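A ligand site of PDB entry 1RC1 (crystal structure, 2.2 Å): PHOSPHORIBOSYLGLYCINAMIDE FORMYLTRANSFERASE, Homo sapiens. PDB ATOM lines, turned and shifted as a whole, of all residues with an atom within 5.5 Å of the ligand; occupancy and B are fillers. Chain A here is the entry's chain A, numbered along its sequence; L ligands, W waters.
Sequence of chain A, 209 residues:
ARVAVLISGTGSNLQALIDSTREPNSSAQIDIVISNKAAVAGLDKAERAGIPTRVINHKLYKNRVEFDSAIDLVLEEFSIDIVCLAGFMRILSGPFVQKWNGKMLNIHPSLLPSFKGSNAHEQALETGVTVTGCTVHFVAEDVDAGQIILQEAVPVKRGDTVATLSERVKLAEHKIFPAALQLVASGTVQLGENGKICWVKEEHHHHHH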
ATOM      1  N   ARG A  64      25.136   6.148   0.347  1.00  0.00           N
ATOM      2  CA  ARG A  64      24.280   7.315   0.232  1.00  0.00           C
ATOM      3  C   ARG A  64      23.445   7.324  -1.056  1.00  0.00           C
ATOM      4  O   ARG A  64      22.231   7.622  -1.027  1.00  0.00           O
ATOM      5  CB  ARG A  64      25.131   8.589   0.301  1.00  0.00           C
ATOM      6  CG  ARG A  64      25.110   9.237   1.653  1.00  0.00           C
ATOM      7  CD  ARG A  64      26.068  10.402   1.818  1.00  0.00           C
ATOM      8  NE  ARG A  64      26.824  10.275   3.059  1.00  0.00           N
ATOM      9  CZ  ARG A  64      26.371  10.552   4.281  1.00  0.00           C
ATOM     10  NH1 ARG A  64      25.129  11.000   4.459  1.00  0.00           N
ATOM     11  NH2 ARG A  64      27.165  10.390   5.328  1.00  0.00           N
ATOM     12  N   LEU A  85      13.661  20.338   3.087  1.00  0.00           N
ATOM     13  CA  LEU A  85      14.355  19.677   4.176  1.00  0.00           C
ATOM     14  C   LEU A  85      14.083  20.412   5.477  1.00  0.00           C
ATOM     15  O   LEU A  85      14.532  21.549   5.665  1.00  0.00           O
ATOM     16  CB  LEU A  85      15.867  19.602   3.922  1.00  0.00           C
ATOM     17  CG  LEU A  85      16.354  19.015   2.587  1.00  0.00           C
ATOM     18  CD1 LEU A  85      17.888  19.004   2.551  1.00  0.00           C
ATOM     19  CD2 LEU A  85      15.820  17.620   2.333  1.00  0.00           C
ATOM     20  N   GLY A  87      14.558  19.866   9.300  1.00  0.00           N
ATOM     21  CA  GLY A  87      15.134  19.043  10.350  1.00  0.00           C
ATOM     22  C   GLY A  87      15.594  17.674   9.870  1.00  0.00           C
ATOM     23  O   GLY A  87      15.724  16.749  10.666  1.00  0.00           O
ATOM     24  N   PHE A  88      15.814  17.538   8.567  1.00  0.00           N
ATOM     25  CA  PHE A  88      16.333  16.318   7.960  1.00  0.00           C
ATOM     26  C   PHE A  88      17.847  16.274   8.185  1.00  0.00           C
ATOM     27  O   PHE A  88      18.553  17.259   7.901  1.00  0.00           O
ATOM     28  CB  PHE A  88      16.035  16.305   6.448  1.00  0.00           C
ATOM     29  CG  PHE A  88      16.418  15.022   5.750  1.00  0.00           C
ATOM     30  CD1 PHE A  88      15.740  13.822   6.027  1.00  0.00           C
ATOM     31  CD2 PHE A  88      17.432  15.011   4.790  1.00  0.00           C
ATOM     32  CE1 PHE A  88      16.077  12.641   5.357  1.00  0.00           C
ATOM     33  CE2 PHE A  88      17.804  13.832   4.125  1.00  0.00           C
ATOM     34  CZ  PHE A  88      17.131  12.640   4.405  1.00  0.00           C
ATOM     35  N   MET A  89      18.333  15.126   8.637  1.00  0.00           N
ATOM     36  CA  MET A  89      19.699  15.037   9.181  1.00  0.00           C
ATOM     37  C   MET A  89      20.724  14.252   8.356  1.00  0.00           C
ATOM     38  O   MET A  89      21.806  13.983   8.846  1.00  0.00           O
ATOM     39  CB  MET A  89      19.659  14.539  10.638  1.00  0.00           C
ATOM     40  CG  MET A  89      19.122  15.585  11.617  1.00  0.00           C
ATOM     41  SD  MET A  89      20.177  17.088  11.713  1.00  0.00           S
ATOM     42  CE  MET A  89      18.966  18.371  11.434  1.00  0.00           C
ATOM     43  N   ARG A  90      20.356  13.890   7.118  1.00  0.00           N
ATOM     44  CA  ARG A  90      21.280  13.189   6.217  1.00  0.00           C
ATOM     45  C   ARG A  90      21.815  14.092   5.110  1.00  0.00           C
ATOM     46  O   ARG A  90      21.043  14.725   4.377  1.00  0.00           O
ATOM     47  CB  ARG A  90      20.590  11.965   5.581  1.00  0.00           C
ATOM     48  CG  ARG A  90      19.940  10.977   6.588  1.00  0.00           C
ATOM     49  CD  ARG A  90      20.898  10.357   7.591  1.00  0.00           C
ATOM     50  NE  ARG A  90      22.054   9.740   6.938  1.00  0.00           N
ATOM     51  CZ  ARG A  90      23.118   9.219   7.561  1.00  0.00           C
ATOM     52  NH1 ARG A  90      23.184   9.222   8.885  1.00  0.00           N
ATOM     53  NH2 ARG A  90      24.099   8.680   6.861  1.00  0.00           N
ATOM     54  N   ILE A  91      23.135  14.142   4.979  1.00  0.00           N
ATOM     55  CA  ILE A  91      23.767  14.787   3.839  1.00  0.00           C
ATOM     56  C   ILE A  91      23.399  13.987   2.594  1.00  0.00           C
ATOM     57  O   ILE A  91      23.510  12.761   2.595  1.00  0.00           O
ATOM     58  CB  ILE A  91      25.314  14.839   4.029  1.00  0.00           C
ATOM     59  CG1 ILE A  91      25.704  15.752   5.215  1.00  0.00           C
ATOM     60  CG2 ILE A  91      26.036  15.246   2.711  1.00  0.00           C
ATOM     61  CD1 ILE A  91      24.796  16.961   5.350  1.00  0.00           C
ATOM     62  N   LEU A  92      22.937  14.674   1.553  1.00  0.00           N
ATOM     63  CA  LEU A  92      22.526  14.016   0.307  1.00  0.00           C
ATOM     64  C   LEU A  92      23.643  14.018  -0.736  1.00  0.00           C
ATOM     65  O   LEU A  92      24.420  14.977  -0.840  1.00  0.00           O
ATOM     66  CB  LEU A  92      21.280  14.695  -0.256  1.00  0.00           C
ATOM     67  CG  LEU A  92      20.035  14.627   0.633  1.00  0.00           C
ATOM     68  CD1 LEU A  92      19.140  15.797   0.318  1.00  0.00           C
ATOM     69  CD2 LEU A  92      19.290  13.290   0.451  1.00  0.00           C
ATOM     70  N   SER A  93      23.696  12.936  -1.517  1.00  0.00           N
ATOM     71  CA  SER A  93      24.736  12.718  -2.527  1.00  0.00           C
ATOM     72  C   SER A  93      24.628  13.715  -3.668  1.00  0.00           C
ATOM     73  O   SER A  93      23.561  14.298  -3.930  1.00  0.00           O
ATOM     74  CB  SER A  93      24.640  11.303  -3.097  1.00  0.00           C
ATOM     75  OG  SER A  93      23.439  11.153  -3.858  1.00  0.00           O
ATOM     76  N   VAL A  97      21.311  15.739  -5.389  1.00  0.00           N
ATOM     77  CA  VAL A  97      21.359  17.189  -5.239  1.00  0.00           C
ATOM     78  C   VAL A  97      21.353  17.863  -6.606  1.00  0.00           C
ATOM     79  O   VAL A  97      20.642  18.857  -6.814  1.00  0.00           O
ATOM     80  CB  VAL A  97      22.617  17.633  -4.400  1.00  0.00           C
ATOM     81  CG1 VAL A  97      22.925  19.125  -4.574  1.00  0.00           C
ATOM     82  CG2 VAL A  97      22.411  17.316  -2.925  1.00  0.00           C
ATOM     83  N   ASN A 106      16.418  24.137   2.208  1.00  0.00           N
ATOM     84  CA  ASN A 106      16.715  23.722   3.586  1.00  0.00           C
ATOM     85  C   ASN A 106      16.595  24.889   4.571  1.00  0.00           C
ATOM     86  O   ASN A 106      16.837  26.050   4.219  1.00  0.00           O
ATOM     87  CB  ASN A 106      18.100  23.078   3.672  1.00  0.00           C
ATOM     88  CG  ASN A 106      18.468  22.665   5.089  1.00  0.00           C
ATOM     89  OD1 ASN A 106      17.900  21.720   5.648  1.00  0.00           O
ATOM     90  ND2 ASN A 106      19.419  23.372   5.682  1.00  0.00           N
ATOM     91  N   ILE A 107      16.194  24.568   5.795  1.00  0.00           N
ATOM     92  CA  ILE A 107      16.173  25.540   6.879  1.00  0.00           C
ATOM     93  C   ILE A 107      17.368  25.239   7.780  1.00  0.00           C
ATOM     94  O   ILE A 107      17.553  24.096   8.212  1.00  0.00           O
ATOM     95  CB  ILE A 107      14.800  25.500   7.660  1.00  0.00           C
ATOM     96  CG1 ILE A 107      14.765  26.560   8.763  1.00  0.00           C
ATOM     97  CG2 ILE A 107      14.551  24.121   8.275  1.00  0.00           C
ATOM     98  CD1 ILE A 107      14.622  28.036   8.293  1.00  0.00           C
ATOM     99  N   HIS A 108      18.189  26.255   8.040  1.00  0.00           N
ATOM    100  CA  HIS A 108      19.368  26.071   8.872  1.00  0.00           C
ATOM    101  C   HIS A 108      19.362  27.106   9.991  1.00  0.00           C
ATOM    102  O   HIS A 108      19.199  28.285   9.698  1.00  0.00           O
ATOM    103  CB  HIS A 108      20.653  26.228   8.037  1.00  0.00           C
ATOM    104  CG  HIS A 108      21.903  26.204   8.864  1.00  0.00           C
ATOM    105  ND1 HIS A 108      22.526  25.039   9.254  1.00  0.00           N
ATOM    106  CD2 HIS A 108      22.624  27.209   9.416  1.00  0.00           C
ATOM    107  CE1 HIS A 108      23.587  25.328   9.981  1.00  0.00           C
ATOM    108  NE2 HIS A 108      23.672  26.632  10.100  1.00  0.00           N
ATOM    109  N   PRO A 109      19.553  26.675  11.245  1.00  0.00           N
ATOM    110  CA  PRO A 109      19.458  27.582  12.403  1.00  0.00           C
ATOM    111  C   PRO A 109      20.704  28.446  12.705  1.00  0.00           C
ATOM    112  O   PRO A 109      21.134  28.541  13.865  1.00  0.00           O
ATOM    113  CB  PRO A 109      19.159  26.607  13.573  1.00  0.00           C
ATOM    114  CG  PRO A 109      19.860  25.333  13.170  1.00  0.00           C
ATOM    115  CD  PRO A 109      19.833  25.282  11.655  1.00  0.00           C
ATOM    116  N   LYS A 116      27.972  26.811  10.087  1.00  0.00           N
ATOM    117  CA  LYS A 116      27.573  25.667   9.275  1.00  0.00           C
ATOM    118  C   LYS A 116      27.620  24.428  10.151  1.00  0.00           C
ATOM    119  O   LYS A 116      28.347  24.405  11.148  1.00  0.00           O
ATOM    120  CB  LYS A 116      28.541  25.468   8.128  1.00  0.00           C
ATOM    121  CG  LYS A 116      28.508  26.588   7.112  1.00  0.00           C
ATOM    122  CD  LYS A 116      29.633  26.350   6.088  1.00  0.00           C
ATOM    123  CE  LYS A 116      29.561  27.366   4.966  1.00  0.00           C
ATOM    124  NZ  LYS A 116      30.498  27.003   3.835  1.00  0.00           N
ATOM    125  N   GLY A 117      26.882  23.387   9.752  1.00  0.00           N
ATOM    126  CA  GLY A 117      26.860  22.125  10.498  1.00  0.00           C
ATOM    127  C   GLY A 117      25.636  22.007  11.385  1.00  0.00           C
ATOM    128  O   GLY A 117      24.895  22.994  11.562  1.00  0.00           O
ATOM    129  N   SER A 118      25.435  20.815  11.942  1.00  0.00           N
ATOM    130  CA  SER A 118      24.236  20.446  12.715  1.00  0.00           C
ATOM    131  C   SER A 118      24.177  20.975  14.154  1.00  0.00           C
ATOM    132  O   SER A 118      23.116  20.914  14.789  1.00  0.00           O
ATOM    133  CB  SER A 118      24.098  18.921  12.763  1.00  0.00           C
ATOM    134  OG  SER A 118      25.307  18.342  13.240  1.00  0.00           O
ATOM    135  N   HIS A 137      17.919  28.205   2.460  1.00  0.00           N
ATOM    136  CA  HIS A 137      18.766  28.238   1.272  1.00  0.00           C
ATOM    137  C   HIS A 137      18.431  27.091   0.327  1.00  0.00           C
ATOM    138  O   HIS A 137      17.888  26.047   0.741  1.00  0.00           O
ATOM    139  CB  HIS A 137      20.246  28.177   1.686  1.00  0.00           C
ATOM    140  CG  HIS A 137      20.590  26.971   2.506  1.00  0.00           C
ATOM    141  ND1 HIS A 137      21.198  25.852   1.972  1.00  0.00           N
ATOM    142  CD2 HIS A 137      20.395  26.709   3.820  1.00  0.00           C
ATOM    143  CE1 HIS A 137      21.365  24.959   2.924  1.00  0.00           C
ATOM    144  NE2 HIS A 137      20.898  25.451   4.054  1.00  0.00           N
ATOM    145  N   VAL A 139      19.592  23.958  -1.726  1.00  0.00           N
ATOM    146  CA  VAL A 139      20.563  22.963  -1.317  1.00  0.00           C
ATOM    147  C   VAL A 139      21.567  22.778  -2.431  1.00  0.00           C
ATOM    148  O   VAL A 139      21.188  22.507  -3.580  1.00  0.00           O
ATOM    149  CB  VAL A 139      19.881  21.634  -0.946  1.00  0.00           C
ATOM    150  CG1 VAL A 139      20.905  20.482  -0.786  1.00  0.00           C
ATOM    151  CG2 VAL A 139      19.057  21.820   0.309  1.00  0.00           C
ATOM    152  N   ALA A 140      22.841  22.981  -2.100  1.00  0.00           N
ATOM    153  CA  ALA A 140      23.944  22.628  -2.982  1.00  0.00           C
ATOM    154  C   ALA A 140      24.707  21.436  -2.389  1.00  0.00           C
ATOM    155  O   ALA A 140      24.514  21.080  -1.228  1.00  0.00           O
ATOM    156  CB  ALA A 140      24.888  23.822  -3.189  1.00  0.00           C
ATOM    157  N   GLU A 141      25.571  20.840  -3.193  1.00  0.00           N
ATOM    158  CA  GLU A 141      26.395  19.706  -2.755  1.00  0.00           C
ATOM    159  C   GLU A 141      27.239  20.052  -1.537  1.00  0.00           C
ATOM    160  O   GLU A 141      27.302  19.291  -0.574  1.00  0.00           O
ATOM    161  CB  GLU A 141      27.289  19.225  -3.900  1.00  0.00           C
ATOM    162  CG  GLU A 141      27.517  17.732  -3.857  1.00  0.00           C
ATOM    163  CD  GLU A 141      28.231  17.208  -5.082  1.00  0.00           C
ATOM    164  OE1 GLU A 141      27.741  17.456  -6.225  1.00  0.00           O
ATOM    165  OE2 GLU A 141      29.262  16.533  -4.899  1.00  0.00           O
ATOM    166  N   ASP A 142      27.870  21.224  -1.608  1.00  0.00           N
ATOM    167  CA  ASP A 142      28.544  21.822  -0.467  1.00  0.00           C
ATOM    168  C   ASP A 142      27.541  22.066   0.656  1.00  0.00           C
ATOM    169  O   ASP A 142      26.549  22.784   0.463  1.00  0.00           O
ATOM    170  CB  ASP A 142      29.189  23.145  -0.912  1.00  0.00           C
ATOM    171  CG  ASP A 142      30.351  23.568  -0.038  1.00  0.00           C
ATOM    172  OD1 ASP A 142      30.808  22.742   0.793  1.00  0.00           O
ATOM    173  OD2 ASP A 142      30.874  24.706  -0.110  1.00  0.00           O
ATOM    174  N   VAL A 143      27.784  21.471   1.811  1.00  0.00           N
ATOM    175  CA  VAL A 143      26.812  21.469   2.907  1.00  0.00           C
ATOM    176  C   VAL A 143      26.611  22.891   3.473  1.00  0.00           C
ATOM    177  O   VAL A 143      27.580  23.600   3.739  1.00  0.00           O
ATOM    178  CB  VAL A 143      27.223  20.493   4.041  1.00  0.00           C
ATOM    179  CG1 VAL A 143      26.301  20.641   5.263  1.00  0.00           C
ATOM    180  CG2 VAL A 143      27.226  19.036   3.540  1.00  0.00           C
ATOM    181  N   ASP A 144      25.356  23.288   3.645  1.00  0.00           N
ATOM    182  CA  ASP A 144      25.002  24.599   4.190  1.00  0.00           C
ATOM    183  C   ASP A 144      25.661  25.743   3.406  1.00  0.00           C
ATOM    184  O   ASP A 144      26.026  26.758   3.995  1.00  0.00           O
ATOM    185  CB  ASP A 144      25.377  24.694   5.696  1.00  0.00           C
ATOM    186  CG  ASP A 144      24.456  23.875   6.584  1.00  0.00           C
ATOM    187  OD1 ASP A 144      23.269  23.702   6.236  1.00  0.00           O
ATOM    188  OD2 ASP A 144      24.825  23.376   7.668  1.00  0.00           O
ATOM    189  N   ALA A 145      25.826  25.567   2.097  1.00  0.00           N
ATOM    190  CA  ALA A 145      26.502  26.587   1.288  1.00  0.00           C
ATOM    191  C   ALA A 145      25.732  26.974   0.020  1.00  0.00           C
ATOM    192  O   ALA A 145      26.247  27.720  -0.800  1.00  0.00           O
ATOM    193  CB  ALA A 145      27.931  26.160   0.953  1.00  0.00           C
HETATM  194  N1  LIG L   1      23.907  13.360  13.825  1.00  0.00           N
HETATM  195  C1  LIG L   1      23.867  12.619  12.728  1.00  0.00           C
HETATM  196  O1  LIG L   1      23.509  11.441  12.671  1.00  0.00           O
HETATM  197  C2  LIG L   1      24.344  13.388  11.553  1.00  0.00           C
HETATM  198  C3  LIG L   1      24.650  12.542  10.310  1.00  0.00           C
HETATM  199  C4  LIG L   1      25.454  13.191   9.235  1.00  0.00           C
HETATM  200  C5  LIG L   1      25.585  12.390   7.879  1.00  0.00           C
HETATM  201  O2  LIG L   1      26.478  11.555   7.801  1.00  0.00           O
HETATM  202  O3  LIG L   1      24.740  12.608   6.834  1.00  0.00           O
HETATM  203  N2  LIG L   1      24.813  14.534   8.946  1.00  0.00           N
HETATM  204  C6  LIG L   1      25.461  15.725   9.190  1.00  0.00           C
HETATM  205  O4  LIG L   1      26.650  15.797   9.483  1.00  0.00           O
HETATM  206  C7  LIG L   1      24.703  16.905   8.892  1.00  0.00           C
HETATM  207  C8  LIG L   1      23.224  16.838   8.725  1.00  0.00           C
HETATM  208  C9  LIG L   1      22.553  17.996   8.304  1.00  0.00           C
HETATM  209  C10 LIG L   1      25.490  18.159   8.655  1.00  0.00           C
HETATM  210  C11 LIG L   1      24.810  19.359   8.235  1.00  0.00           C
HETATM  211  C12 LIG L   1      23.277  19.259   8.049  1.00  0.00           C
HETATM  212  C13 LIG L   1      22.152  20.388   7.771  1.00  0.00           C
HETATM  213  C14 LIG L   1      21.876  21.720   8.523  1.00  0.00           C
HETATM  214  C15 LIG L   1      21.012  21.321   9.708  1.00  0.00           C
HETATM  215  F1  LIG L   1      21.427  20.224  10.418  1.00  0.00           F
HETATM  216  F2  LIG L   1      19.988  20.826   9.024  1.00  0.00           F
HETATM  217  F3  LIG L   1      20.706  22.394  10.460  1.00  0.00           F
HETATM  218  O5  LIG L   1      21.703  22.751   7.963  1.00  0.00           O
HETATM  219  O6  LIG L   1      23.257  21.897   9.313  1.00  0.00           O
HETATM  220  C16 LIG L   1      21.366  20.436   6.442  1.00  0.00           C
HETATM  221  C17 LIG L   1      22.269  19.965   5.126  1.00  0.00           C
HETATM  222  C18 LIG L   1      21.435  20.423   3.872  1.00  0.00           C
HETATM  223  C19 LIG L   1      22.090  19.500   2.909  1.00  0.00           C
HETATM  224  C20 LIG L   1      22.069  18.094   2.518  1.00  0.00           C
HETATM  225  N3  LIG L   1      21.201  17.238   3.144  1.00  0.00           N
HETATM  226  C21 LIG L   1      22.997  20.194   2.199  1.00  0.00           C
HETATM  227  O7  LIG L   1      23.313  21.545   2.130  1.00  0.00           O
HETATM  228  N4  LIG L   1      23.966  19.611   1.066  1.00  0.00           N
HETATM  229  C22 LIG L   1      23.841  18.278   0.818  1.00  0.00           C
HETATM  230  N5  LIG L   1      24.673  17.637  -0.038  1.00  0.00           N
HETATM  231  N6  LIG L   1      22.956  17.587   1.492  1.00  0.00           N
HETATM  232  O   HOH W   1      22.489  23.371  13.241  1.00  0.00           O
HETATM  233  O   HOH W   2      20.237  21.717  13.470  1.00  0.00           O
HETATM  234  O   HOH W   3      23.948  23.558   0.476  1.00  0.00           O
HETATM  235  O   HOH W   4      16.876  21.514   9.105  1.00  0.00           O
HETATM  236  O   HOH W   5      28.947  15.598   8.109  1.00  0.00           O
HETATM  237  O   HOH W   6      17.386  19.774   7.187  1.00  0.00           O
HETATM  238  O   HOH W   7      27.719  16.648  11.652  1.00  0.00           O
HETATM  239  O   HOH W   8      20.055  17.097   5.506  1.00  0.00           O
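N4 of the ligand lies close to O of Ala 140, at 2.8 Å.
Leu 85 touches the ligand (CD1 to N3, 3.8 Å).
Val 97 touches the ligand.
Pro 109 touches the ligand.
Ser 118 touches the ligand (N to O6, 3.6 Å).
Val 139 touches the ligand.
Asp 142 touches the ligand.
Val 143 touches the ligand (CG1 to C11, 3.6 Å).
Hydrophobic or aromatic side chains that line the ligand: Leu 85, Met 89, Ile 91, Leu 92, Val 97, His 108, Pro 109, Val 139 and Val 143.
18 residues have an atom within 4 Å of the ligand: Arg 64, Leu 85, Met 89, Arg 90, Ile 91, Leu 92, Val 97, Asn 106, His 108, Pro 109, Gly 117, Ser 118, Val 139, Ala 140, Glu 141, Asp 142, Val 143 and Asp 144.
The nearest printed residue that does not touch the ligand is Phe 88 (4.01 Å).
Water W7 lies within hydrogen-bond range of O4 of the ligand and OG of Ser 118.
Water W8 lies within hydrogen-bond range of a nitrogen (N3) of the ligand (2.6 Å), the backbone carbonyl oxygen of Arg 90 (2.8 Å) and the backbone carbonyl oxygen of Phe 88 (2.8 Å).
Water W4 bridges O of Ile 107 and N of Gly 87.
Water W6 bridges OD1 of Asn 106 and O of Phe 88.
The side-chain carboxylate (OD2) of Asp 144 is in hydrogen-bond range of a ring nitrogen (ND1) of His 108 (3.3 Å).
The side-chain carboxylate (OD2) of Asp 144 sits at hydrogen-bond distance from the backbone NH (N) of Gly 117 (2.9 Å).
The guanidinium group (NH1) of Arg 64 sits at hydrogen-bond distance from the backbone carbonyl oxygen (O) of Ile 91 (3.0 Å).
The backbone carbonyl oxygen (O) of Leu 85 lies close to the side-chain amide oxygen (OD1) of Asn 106 (3.4 Å).
N of Asn 106 lies within hydrogen-bond range of O of His 137 (2.8 Å).
N of Ile 107 sits at hydrogen-bond distance from O of Leu 85 (3.4 Å).
The backbone NH (N) of Asp 144 sits at hydrogen-bond distance from an oxygen (O7) of the ligand, at 3.1 Å.
An oxygen (O5) of the ligand sits at hydrogen-bond distance from the side-chain carboxylate of Asp 144 (2.5 Å).
O5 of the ligand lies within hydrogen-bond range of ND1 of His 108 (2.8 Å).
The backbone NH (N) of Leu 92 is in hydrogen-bond range of a nitrogen (N6) of the ligand.
A nitrogen (N5) of the ligand is in hydrogen-bond range of the backbone carbonyl oxygen (O) of Leu 92 (2.8 Å).
The backbone carbonyl oxygen (O) of Arg 90 is in hydrogen-bond range of a nitrogen (N3) of the ligand (2.8 Å).
The guanidinium group of Arg 90 is in salt-bridge range of an oxygen (O2) of the ligand (3.8 Å).
NH2 of Arg 64 lies within salt-bridge range of O2 of the ligand (2.8 Å).
The backbone NH (N) of Ile 91 sits at hydrogen-bond distance from an oxygen (O3) of the ligand (2.9 Å).
O of Gly 117 is in hydrogen-bond range of O6 of the ligand (3.0 Å).
A nitrogen (N2) of the ligand is in hydrogen-bond range of the backbone carbonyl oxygen (O) of Met 89, at 3.1 Å.
A nitrogen (N5) of the ligand is in hydrogen-bond range of the backbone carbonyl oxygen (O) of Glu 141 (3.2 Å).
The side-chain amide nitrogen (ND2) of Asn 106 sits at hydrogen-bond distance from an oxygen (O5) of the ligand (3.3 Å).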
